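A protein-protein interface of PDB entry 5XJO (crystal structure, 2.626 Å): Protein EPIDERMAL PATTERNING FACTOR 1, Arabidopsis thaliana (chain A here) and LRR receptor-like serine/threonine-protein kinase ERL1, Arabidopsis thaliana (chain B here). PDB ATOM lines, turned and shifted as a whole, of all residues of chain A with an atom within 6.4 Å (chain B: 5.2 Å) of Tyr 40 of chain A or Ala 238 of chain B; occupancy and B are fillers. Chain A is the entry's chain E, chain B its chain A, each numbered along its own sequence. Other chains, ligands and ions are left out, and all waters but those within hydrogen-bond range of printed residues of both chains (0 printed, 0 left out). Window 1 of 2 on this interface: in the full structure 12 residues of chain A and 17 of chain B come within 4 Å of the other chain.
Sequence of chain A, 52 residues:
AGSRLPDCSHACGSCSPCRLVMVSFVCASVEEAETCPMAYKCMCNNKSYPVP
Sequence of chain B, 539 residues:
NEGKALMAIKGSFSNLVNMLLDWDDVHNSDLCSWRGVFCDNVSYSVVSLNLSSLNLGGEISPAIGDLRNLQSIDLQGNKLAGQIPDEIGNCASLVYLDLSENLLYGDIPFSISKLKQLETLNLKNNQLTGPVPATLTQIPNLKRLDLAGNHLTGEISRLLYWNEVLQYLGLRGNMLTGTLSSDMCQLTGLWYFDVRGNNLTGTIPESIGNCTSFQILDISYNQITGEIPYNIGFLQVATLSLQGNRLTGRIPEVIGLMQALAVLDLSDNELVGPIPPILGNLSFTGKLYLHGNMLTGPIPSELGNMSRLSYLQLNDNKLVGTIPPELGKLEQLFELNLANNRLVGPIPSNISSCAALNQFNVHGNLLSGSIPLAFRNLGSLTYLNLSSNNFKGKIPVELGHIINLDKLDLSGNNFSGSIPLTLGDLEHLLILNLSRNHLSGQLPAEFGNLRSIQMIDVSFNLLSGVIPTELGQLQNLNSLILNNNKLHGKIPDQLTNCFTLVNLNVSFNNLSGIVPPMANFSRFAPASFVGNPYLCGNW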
ATOM      1  N   LEU A   5      21.612 -18.848  18.507  1.00  0.00           N
ATOM      2  CA  LEU A   5      20.674 -17.861  18.059  1.00  0.00           C
ATOM      3  C   LEU A   5      20.501 -16.795  19.120  1.00  0.00           C
ATOM      4  O   LEU A   5      20.228 -17.118  20.228  1.00  0.00           O
ATOM      5  CB  LEU A   5      19.375 -18.576  17.818  1.00  0.00           C
ATOM      6  CG  LEU A   5      18.209 -17.755  17.354  1.00  0.00           C
ATOM      7  CD1 LEU A   5      18.521 -17.292  15.966  1.00  0.00           C
ATOM      8  CD2 LEU A   5      16.963 -18.606  17.369  1.00  0.00           C
ATOM      9  N   PRO A   6      20.657 -15.510  18.791  1.00  0.00           N
ATOM     10  CA  PRO A   6      20.531 -14.476  19.834  1.00  0.00           C
ATOM     11  C   PRO A   6      19.184 -14.528  20.533  1.00  0.00           C
ATOM     12  O   PRO A   6      18.138 -14.671  19.907  1.00  0.00           O
ATOM     13  CB  PRO A   6      20.725 -13.161  19.064  1.00  0.00           C
ATOM     14  CG  PRO A   6      21.560 -13.498  17.930  1.00  0.00           C
ATOM     15  CD  PRO A   6      21.344 -14.976  17.600  1.00  0.00           C
ATOM     16  N   LEU A  20      12.986 -11.627  18.561  1.00  0.00           N
ATOM     17  CA  LEU A  20      13.908 -11.627  17.433  1.00  0.00           C
ATOM     18  C   LEU A  20      13.187 -11.610  16.089  1.00  0.00           C
ATOM     19  O   LEU A  20      12.173 -12.293  15.901  1.00  0.00           O
ATOM     20  CB  LEU A  20      14.803 -12.853  17.524  1.00  0.00           C
ATOM     21  CG  LEU A  20      15.782 -13.227  16.421  1.00  0.00           C
ATOM     22  CD1 LEU A  20      16.553 -12.065  15.829  1.00  0.00           C
ATOM     23  CD2 LEU A  20      16.752 -14.101  17.141  1.00  0.00           C
ATOM     24  N   VAL A  21      13.725 -10.818  15.148  1.00  0.00           N
ATOM     25  CA  VAL A  21      13.182 -10.660  13.794  1.00  0.00           C
ATOM     26  C   VAL A  21      14.353 -10.460  12.833  1.00  0.00           C
ATOM     27  O   VAL A  21      15.329  -9.769  13.149  1.00  0.00           O
ATOM     28  CB  VAL A  21      12.155  -9.500  13.675  1.00  0.00           C
ATOM     29  CG1 VAL A  21      11.072  -9.565  14.770  1.00  0.00           C
ATOM     30  CG2 VAL A  21      12.832  -8.135  13.649  1.00  0.00           C
ATOM     31  N   MET A  22      14.280 -11.085  11.666  1.00  0.00           N
ATOM     32  CA  MET A  22      15.438 -11.020  10.787  1.00  0.00           C
ATOM     33  C   MET A  22      15.336  -9.915   9.742  1.00  0.00           C
ATOM     34  O   MET A  22      14.263  -9.395   9.436  1.00  0.00           O
ATOM     35  CB  MET A  22      15.675 -12.365  10.105  1.00  0.00           C
ATOM     36  CG  MET A  22      15.909 -13.457  11.105  1.00  0.00           C
ATOM     37  SD  MET A  22      16.878 -14.797  10.423  1.00  0.00           S
ATOM     38  CE  MET A  22      17.895 -13.937   9.212  1.00  0.00           C
ATOM     39  N   VAL A  23      16.501  -9.553   9.218  1.00  0.00           N
ATOM     40  CA  VAL A  23      16.691  -8.394   8.361  1.00  0.00           C
ATOM     41  C   VAL A  23      17.454  -8.839   7.123  1.00  0.00           C
ATOM     42  O   VAL A  23      18.451  -9.574   7.221  1.00  0.00           O
ATOM     43  CB  VAL A  23      17.454  -7.260   9.099  1.00  0.00           C
ATOM     44  CG1 VAL A  23      17.755  -6.077   8.173  1.00  0.00           C
ATOM     45  CG2 VAL A  23      16.659  -6.773  10.285  1.00  0.00           C
ATOM     46  N   MET A  38      21.869 -11.706   5.286  1.00  0.00           N
ATOM     47  CA  MET A  38      20.897 -11.669   6.367  1.00  0.00           C
ATOM     48  C   MET A  38      21.580 -11.471   7.711  1.00  0.00           C
ATOM     49  O   MET A  38      22.655 -12.028   7.962  1.00  0.00           O
ATOM     50  CB  MET A  38      20.087 -12.966   6.376  1.00  0.00           C
ATOM     51  CG  MET A  38      19.450 -13.300   5.039  1.00  0.00           C
ATOM     52  SD  MET A  38      17.904 -14.151   5.267  1.00  0.00           S
ATOM     53  CE  MET A  38      16.753 -12.803   5.500  1.00  0.00           C
ATOM     54  N   ALA A  39      20.952 -10.648   8.562  1.00  0.00           N
ATOM     55  CA  ALA A  39      21.408 -10.416   9.930  1.00  0.00           C
ATOM     56  C   ALA A  39      20.186 -10.311  10.842  1.00  0.00           C
ATOM     57  O   ALA A  39      19.068 -10.052  10.385  1.00  0.00           O
ATOM     58  CB  ALA A  39      22.268  -9.151  10.012  1.00  0.00           C
ATOM     59  N   TYR A  40      20.403 -10.471  12.143  1.00  0.00           N
ATOM     60  CA  TYR A  40      19.311 -10.490  13.119  1.00  0.00           C
ATOM     61  C   TYR A  40      19.177  -9.157  13.857  1.00  0.00           C
ATOM     62  O   TYR A  40      20.162  -8.457  14.084  1.00  0.00           O
ATOM     63  CB  TYR A  40      19.521 -11.598  14.157  1.00  0.00           C
ATOM     64  CG  TYR A  40      19.667 -13.018  13.655  1.00  0.00           C
ATOM     65  CD1 TYR A  40      18.570 -13.881  13.664  1.00  0.00           C
ATOM     66  CD2 TYR A  40      20.907 -13.532  13.266  1.00  0.00           C
ATOM     67  CE1 TYR A  40      18.676 -15.207  13.253  1.00  0.00           C
ATOM     68  CE2 TYR A  40      21.033 -14.859  12.828  1.00  0.00           C
ATOM     69  CZ  TYR A  40      19.913 -15.701  12.832  1.00  0.00           C
ATOM     70  OH  TYR A  40      20.012 -17.040  12.411  1.00  0.00           O
ATOM     71  N   LYS A  41      17.948  -8.815  14.249  1.00  0.00           N
ATOM     72  CA  LYS A  41      17.750  -7.714  15.192  1.00  0.00           C
ATOM     73  C   LYS A  41      16.710  -8.122  16.233  1.00  0.00           C
ATOM     74  O   LYS A  41      15.990  -9.115  16.067  1.00  0.00           O
ATOM     75  CB  LYS A  41      17.330  -6.406  14.485  1.00  0.00           C
ATOM     76  CG  LYS A  41      18.187  -5.975  13.269  1.00  0.00           C
ATOM     77  CD  LYS A  41      19.588  -5.438  13.614  1.00  0.00           C
ATOM     78  CE  LYS A  41      20.413  -5.169  12.327  1.00  0.00           C
ATOM     79  NZ  LYS A  41      21.833  -4.709  12.523  1.00  0.00           N
ATOM     80  N   CYS A  42      16.633  -7.351  17.321  1.00  0.00           N
ATOM     81  CA  CYS A  42      15.562  -7.495  18.311  1.00  0.00           C
ATOM     82  C   CYS A  42      14.542  -6.382  18.115  1.00  0.00           C
ATOM     83  O   CYS A  42      14.906  -5.246  17.822  1.00  0.00           O
ATOM     84  CB  CYS A  42      16.082  -7.434  19.755  1.00  0.00           C
ATOM     85  SG  CYS A  42      17.292  -8.685  20.289  1.00  0.00           S
ATOM     86  N   TYR A  49      16.267  -2.816  17.982  1.00  0.00           N
ATOM     87  CA  TYR A  49      17.375  -2.879  18.925  1.00  0.00           C
ATOM     88  C   TYR A  49      18.363  -3.912  18.410  1.00  0.00           C
ATOM     89  O   TYR A  49      17.998  -4.774  17.604  1.00  0.00           O
ATOM     90  CB  TYR A  49      16.941  -3.267  20.346  1.00  0.00           C
ATOM     91  CG  TYR A  49      15.932  -2.369  20.992  1.00  0.00           C
ATOM     92  CD1 TYR A  49      14.581  -2.489  20.713  1.00  0.00           C
ATOM     93  CD2 TYR A  49      16.333  -1.414  21.903  1.00  0.00           C
ATOM     94  CE1 TYR A  49      13.662  -1.670  21.324  1.00  0.00           C
ATOM     95  CE2 TYR A  49      15.431  -0.594  22.510  1.00  0.00           C
ATOM     96  CZ  TYR A  49      14.102  -0.720  22.225  1.00  0.00           C
ATOM     97  OH  TYR A  49      13.233   0.118  22.863  1.00  0.00           O
ATOM     98  N   PRO A  50      19.626  -3.840  18.834  1.00  0.00           N
ATOM     99  CA  PRO A  50      20.590  -4.856  18.412  1.00  0.00           C
ATOM    100  C   PRO A  50      20.562  -6.102  19.293  1.00  0.00           C
ATOM    101  O   PRO A  50      20.301  -6.059  20.496  1.00  0.00           O
ATOM    102  CB  PRO A  50      21.937  -4.124  18.519  1.00  0.00           C
ATOM    103  CG  PRO A  50      21.635  -2.767  19.170  1.00  0.00           C
ATOM    104  CD  PRO A  50      20.258  -2.806  19.682  1.00  0.00           C
ATOM    105  N   VAL A  51      20.863  -7.234  18.657  1.00  0.00           N
ATOM    106  CA  VAL A  51      20.911  -8.542  19.312  1.00  0.00           C
ATOM    107  C   VAL A  51      22.065  -8.578  20.308  1.00  0.00           C
ATOM    108  O   VAL A  51      23.088  -7.933  20.060  1.00  0.00           O
ATOM    109  CB  VAL A  51      21.048  -9.660  18.264  1.00  0.00           C
ATOM    110  CG1 VAL A  51      19.994  -9.494  17.191  1.00  0.00           C
ATOM    111  CG2 VAL A  51      22.448  -9.684  17.636  1.00  0.00           C
ATOM    112  N   PHE B 214      31.294  -9.644  13.762  1.00  0.00           N
ATOM    113  CA  PHE B 214      30.800  -9.665  12.399  1.00  0.00           C
ATOM    114  C   PHE B 214      29.397 -10.286  12.372  1.00  0.00           C
ATOM    115  O   PHE B 214      29.178 -11.375  12.907  1.00  0.00           O
ATOM    116  CB  PHE B 214      31.751 -10.461  11.500  1.00  0.00           C
ATOM    117  CG  PHE B 214      33.090  -9.803  11.227  1.00  0.00           C
ATOM    118  CD1 PHE B 214      33.471  -8.622  11.845  1.00  0.00           C
ATOM    119  CD2 PHE B 214      33.991 -10.401  10.344  1.00  0.00           C
ATOM    120  CE1 PHE B 214      34.725  -8.070  11.585  1.00  0.00           C
ATOM    121  CE2 PHE B 214      35.222  -9.844  10.078  1.00  0.00           C
ATOM    122  CZ  PHE B 214      35.589  -8.680  10.692  1.00  0.00           C
ATOM    123  N   GLN B 215      28.432  -9.580  11.786  1.00  0.00           N
ATOM    124  CA  GLN B 215      27.185 -10.225  11.419  1.00  0.00           C
ATOM    125  C   GLN B 215      27.208 -10.790  10.000  1.00  0.00           C
ATOM    126  O   GLN B 215      26.594 -11.834   9.748  1.00  0.00           O
ATOM    127  CB  GLN B 215      26.043  -9.233  11.578  1.00  0.00           C
ATOM    128  CG  GLN B 215      26.023  -8.594  12.953  1.00  0.00           C
ATOM    129  CD  GLN B 215      24.711  -7.878  13.213  1.00  0.00           C
ATOM    130  OE1 GLN B 215      23.632  -8.355  12.799  1.00  0.00           O
ATOM    131  NE2 GLN B 215      24.779  -6.747  13.931  1.00  0.00           N
ATOM    132  N   ILE B 216      27.943 -10.157   9.076  1.00  0.00           N
ATOM    133  CA  ILE B 216      28.055 -10.596   7.687  1.00  0.00           C
ATOM    134  C   ILE B 216      29.522 -10.691   7.320  1.00  0.00           C
ATOM    135  O   ILE B 216      30.269  -9.714   7.461  1.00  0.00           O
ATOM    136  CB  ILE B 216      27.330  -9.641   6.719  1.00  0.00           C
ATOM    137  CG1 ILE B 216      25.829  -9.639   7.041  1.00  0.00           C
ATOM    138  CG2 ILE B 216      27.558 -10.093   5.304  1.00  0.00           C
ATOM    139  CD1 ILE B 216      25.181  -8.262   7.085  1.00  0.00           C
ATOM    140  N   GLN B 236      30.258 -15.308  15.102  1.00  0.00           N
ATOM    141  CA  GLN B 236      28.845 -15.154  15.418  1.00  0.00           C
ATOM    142  C   GLN B 236      28.076 -14.548  14.259  1.00  0.00           C
ATOM    143  O   GLN B 236      27.025 -13.933  14.472  1.00  0.00           O
ATOM    144  CB  GLN B 236      28.683 -14.311  16.672  1.00  0.00           C
ATOM    145  CG  GLN B 236      29.709 -14.679  17.725  1.00  0.00           C
ATOM    146  CD  GLN B 236      29.248 -15.854  18.549  1.00  0.00           C
ATOM    147  OE1 GLN B 236      28.220 -15.759  19.215  1.00  0.00           O
ATOM    148  NE2 GLN B 236      29.949 -16.993  18.446  1.00  0.00           N
ATOM    149  N   VAL B 237      28.592 -14.736  13.040  1.00  0.00           N
ATOM    150  CA  VAL B 237      27.965 -14.224  11.841  1.00  0.00           C
ATOM    151  C   VAL B 237      26.622 -14.910  11.601  1.00  0.00           C
ATOM    152  O   VAL B 237      26.435 -16.102  11.886  1.00  0.00           O
ATOM    153  CB  VAL B 237      28.903 -14.435  10.636  1.00  0.00           C
ATOM    154  CG1 VAL B 237      30.047 -13.428  10.639  1.00  0.00           C
ATOM    155  CG2 VAL B 237      29.451 -15.878  10.628  1.00  0.00           C
ATOM    156  N   ALA B 238      25.691 -14.157  11.019  1.00  0.00           N
ATOM    157  CA  ALA B 238      24.489 -14.758  10.454  1.00  0.00           C
ATOM    158  C   ALA B 238      24.731 -15.278   9.040  1.00  0.00           C
ATOM    159  O   ALA B 238      24.245 -16.357   8.686  1.00  0.00           O
ATOM    160  CB  ALA B 238      23.353 -13.741  10.436  1.00  0.00           C
ATOM    161  N   THR B 239      25.462 -14.514   8.226  1.00  0.00           N
ATOM    162  CA  THR B 239      25.733 -14.840   6.837  1.00  0.00           C
ATOM    163  C   THR B 239      27.221 -15.104   6.642  1.00  0.00           C
ATOM    164  O   THR B 239      28.053 -14.199   6.826  1.00  0.00           O
ATOM    165  CB  THR B 239      25.309 -13.713   5.898  1.00  0.00           C
ATOM    166  OG1 THR B 239      23.898 -13.468   5.992  1.00  0.00           O
ATOM    167  CG2 THR B 239      25.645 -14.132   4.476  1.00  0.00           C
ATOM    168  N   LEU B 240      27.547 -16.323   6.221  1.00  0.00           N
ATOM    169  CA  LEU B 240      28.924 -16.704   5.943  1.00  0.00           C
ATOM    170  C   LEU B 240      28.968 -17.041   4.457  1.00  0.00           C
ATOM    171  O   LEU B 240      28.569 -18.139   4.045  1.00  0.00           O
ATOM    172  CB  LEU B 240      29.380 -17.882   6.802  1.00  0.00           C
ATOM    173  CG  LEU B 240      30.812 -18.363   6.520  1.00  0.00           C
ATOM    174  CD1 LEU B 240      31.818 -17.256   6.809  1.00  0.00           C
ATOM    175  CD2 LEU B 240      31.146 -19.622   7.301  1.00  0.00           C
ATOM    176  N   GLN B 259      25.068 -22.251  15.282  1.00  0.00           N
ATOM    177  CA  GLN B 259      23.612 -22.189  15.211  1.00  0.00           C
ATOM    178  C   GLN B 259      23.086 -20.796  14.895  1.00  0.00           C
ATOM    179  O   GLN B 259      21.932 -20.670  14.488  1.00  0.00           O
ATOM    180  CB  GLN B 259      22.977 -22.700  16.524  1.00  0.00           C
ATOM    181  CG  GLN B 259      23.151 -24.196  16.723  1.00  0.00           C
ATOM    182  CD  GLN B 259      22.327 -24.771  17.849  1.00  0.00           C
ATOM    183  OE1 GLN B 259      21.782 -24.048  18.701  1.00  0.00           O
ATOM    184  NE2 GLN B 259      22.218 -26.094  17.866  1.00  0.00           N
ATOM    185  N   ALA B 260      23.900 -19.759  15.017  1.00  0.00           N
ATOM    186  CA  ALA B 260      23.442 -18.436  14.637  1.00  0.00           C
ATOM    187  C   ALA B 260      23.385 -18.239  13.138  1.00  0.00           C
ATOM    188  O   ALA B 260      22.920 -17.183  12.702  1.00  0.00           O
ATOM    189  CB  ALA B 260      24.357 -17.366  15.236  1.00  0.00           C
ATOM    190  N   LEU B 261      23.879 -19.194  12.352  1.00  0.00           N
ATOM    191  CA  LEU B 261      23.912 -19.032  10.900  1.00  0.00           C
ATOM    192  C   LEU B 261      22.517 -18.873  10.314  1.00  0.00           C
ATOM    193  O   LEU B 261      21.640 -19.707  10.543  1.00  0.00           O
ATOM    194  CB  LEU B 261      24.581 -20.234  10.241  1.00  0.00           C
ATOM    195  CG  LEU B 261      26.094 -20.230  10.160  1.00  0.00           C
ATOM    196  CD1 LEU B 261      26.470 -21.431   9.332  1.00  0.00           C
ATOM    197  CD2 LEU B 261      26.614 -18.938   9.528  1.00  0.00           C
ATOM    198  N   ALA B 262      22.313 -17.808   9.546  1.00  0.00           N
ATOM    199  CA  ALA B 262      21.093 -17.698   8.761  1.00  0.00           C
ATOM    200  C   ALA B 262      21.295 -18.148   7.330  1.00  0.00           C
ATOM    201  O   ALA B 262      20.365 -18.676   6.718  1.00  0.00           O
ATOM    202  CB  ALA B 262      20.557 -16.267   8.766  1.00  0.00           C
ATOM    203  N   VAL B 263      22.500 -17.951   6.796  1.00  0.00           N
ATOM    204  CA  VAL B 263      22.831 -18.231   5.407  1.00  0.00           C
ATOM    205  C   VAL B 263      24.251 -18.765   5.391  1.00  0.00           C
ATOM    206  O   VAL B 263      25.187 -18.039   5.754  1.00  0.00           O
ATOM    207  CB  VAL B 263      22.746 -16.979   4.508  1.00  0.00           C
ATOM    208  CG1 VAL B 263      23.245 -17.322   3.108  1.00  0.00           C
ATOM    209  CG2 VAL B 263      21.352 -16.394   4.453  1.00  0.00           C
ATOM    210  N   PHE B 284      18.184 -23.604  12.819  1.00  0.00           N
ATOM    211  CA  PHE B 284      17.731 -22.243  12.568  1.00  0.00           C
ATOM    212  C   PHE B 284      18.226 -21.689  11.233  1.00  0.00           C
ATOM    213  O   PHE B 284      17.837 -20.576  10.855  1.00  0.00           O
ATOM    214  CB  PHE B 284      18.182 -21.309  13.710  1.00  0.00           C
ATOM    215  CG  PHE B 284      18.068 -21.919  15.088  1.00  0.00           C
ATOM    216  CD1 PHE B 284      16.835 -21.977  15.753  1.00  0.00           C
ATOM    217  CD2 PHE B 284      19.201 -22.409  15.743  1.00  0.00           C
ATOM    218  CE1 PHE B 284      16.739 -22.536  17.036  1.00  0.00           C
ATOM    219  CE2 PHE B 284      19.106 -22.968  17.033  1.00  0.00           C
ATOM    220  CZ  PHE B 284      17.875 -23.030  17.678  1.00  0.00           C
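The backbone NH of Ala 238 of chain B lies within hydrogen-bond range of the backbone carbonyl oxygen of Gln 215 of chain B, at 2.8 Å. The backbone carbonyl oxygen of Gln 215 of chain B is in hydrogen-bond range of the backbone NH of Thr 239 of chain B. The backbone carbonyl oxygen (O) of Ala 238 of chain B sits at hydrogen-bond distance from the backbone NH (N) of Ala 262 of chain B. N of Val 263 of chain B is in hydrogen-bond range of O of Ala 238 of chain B. N of Leu 240 of chain B sits at hydrogen-bond distance from O of Val 263 of chain B, 3.0 Å away. The backbone carbonyl oxygen (O) of Ala 39 of chain A sits at hydrogen-bond distance from the backbone NH (N) of Val 23 of chain A.
Of chain B, only Gln 215 (3.7 Å), Ala 238 (3.5 Å), Ala 260 (2.9 Å), Leu 261 (3.6 Å) and Ala 262 (3.8 Å) come within 4 Å of Tyr 40 of chain A. Ala 238 of chain B touches three residues of chain A. Of the printed residues of chain B, Lys 41 of chain A touches Gln 215. Printed residues of chain A within 4 Å of Thr 239 of chain B: Met 38 (2.7 Å). Of the printed residues of chain A, Leu 261 of chain B touches Tyr 40. Leu 240 of chain B touches none of the printed residues of chain A. The nearest residue of chain B that does not touch Tyr 40 of chain A is Phe 284 of chain B (4.4 Å). The nearest residue of chain A that does not touch Ala 238 of chain B is Met 22 of chain A (5.6 Å). The nearest printed residue of chain A that does not touch Ala 260 of chain B is Leu 5 of chain A (4.3 Å).
The side-chain hydroxyl (OG1) of Thr 239 of chain B sits at hydrogen-bond distance from the backbone carbonyl oxygen (O) of Met 38 of chain A, at 2.7 Å. The side-chain hydroxyl (OH) of Tyr 40 of chain A sits at hydrogen-bond distance from the backbone carbonyl oxygen (O) of Ala 260 of chain B, at 2.9 Å.
Of the 14 printed residues of chain B, 8 touch a printed residue of chain A. Hydrophobic or aromatic side chains of chain A that line the printed part of chain B: Leu 5, Met 22, Met 38, Ala 39 and Tyr 40. Among the printed residues, no Asp or Glu carboxylate lies within 4 Å of a Lys or Arg side-chain nitrogen of the other chain.
Among the printed residues, pairs that only touch across the chains: Met 38 of chain A with Ala 238 of chain B (3.1 Å), Ala 39 of chain A with Gln 215 of chain B (3.2 Å), Tyr 40 of chain A with Ala 238 of chain B (3.5 Å), Met 22 of chain A with Ala 262 of chain B (3.6 Å), Tyr 40 of chain A with Leu 261 of chain B (3.6 Å), Met 38 of chain A with Val 263 of chain B (3.7 Å), Tyr 40 of chain A with Gln 215 of chain B (3.7 Å), Leu 5 of chain A with Phe 284 of chain B (3.7 Å), Tyr 40 of chain A with Ala 262 of chain B (3.8 Å), Lys 41 of chain A with Gln 215 of chain B (3.8 Å) and Ala 39 of chain A with Ala 238 of chain B (3.9 Å).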
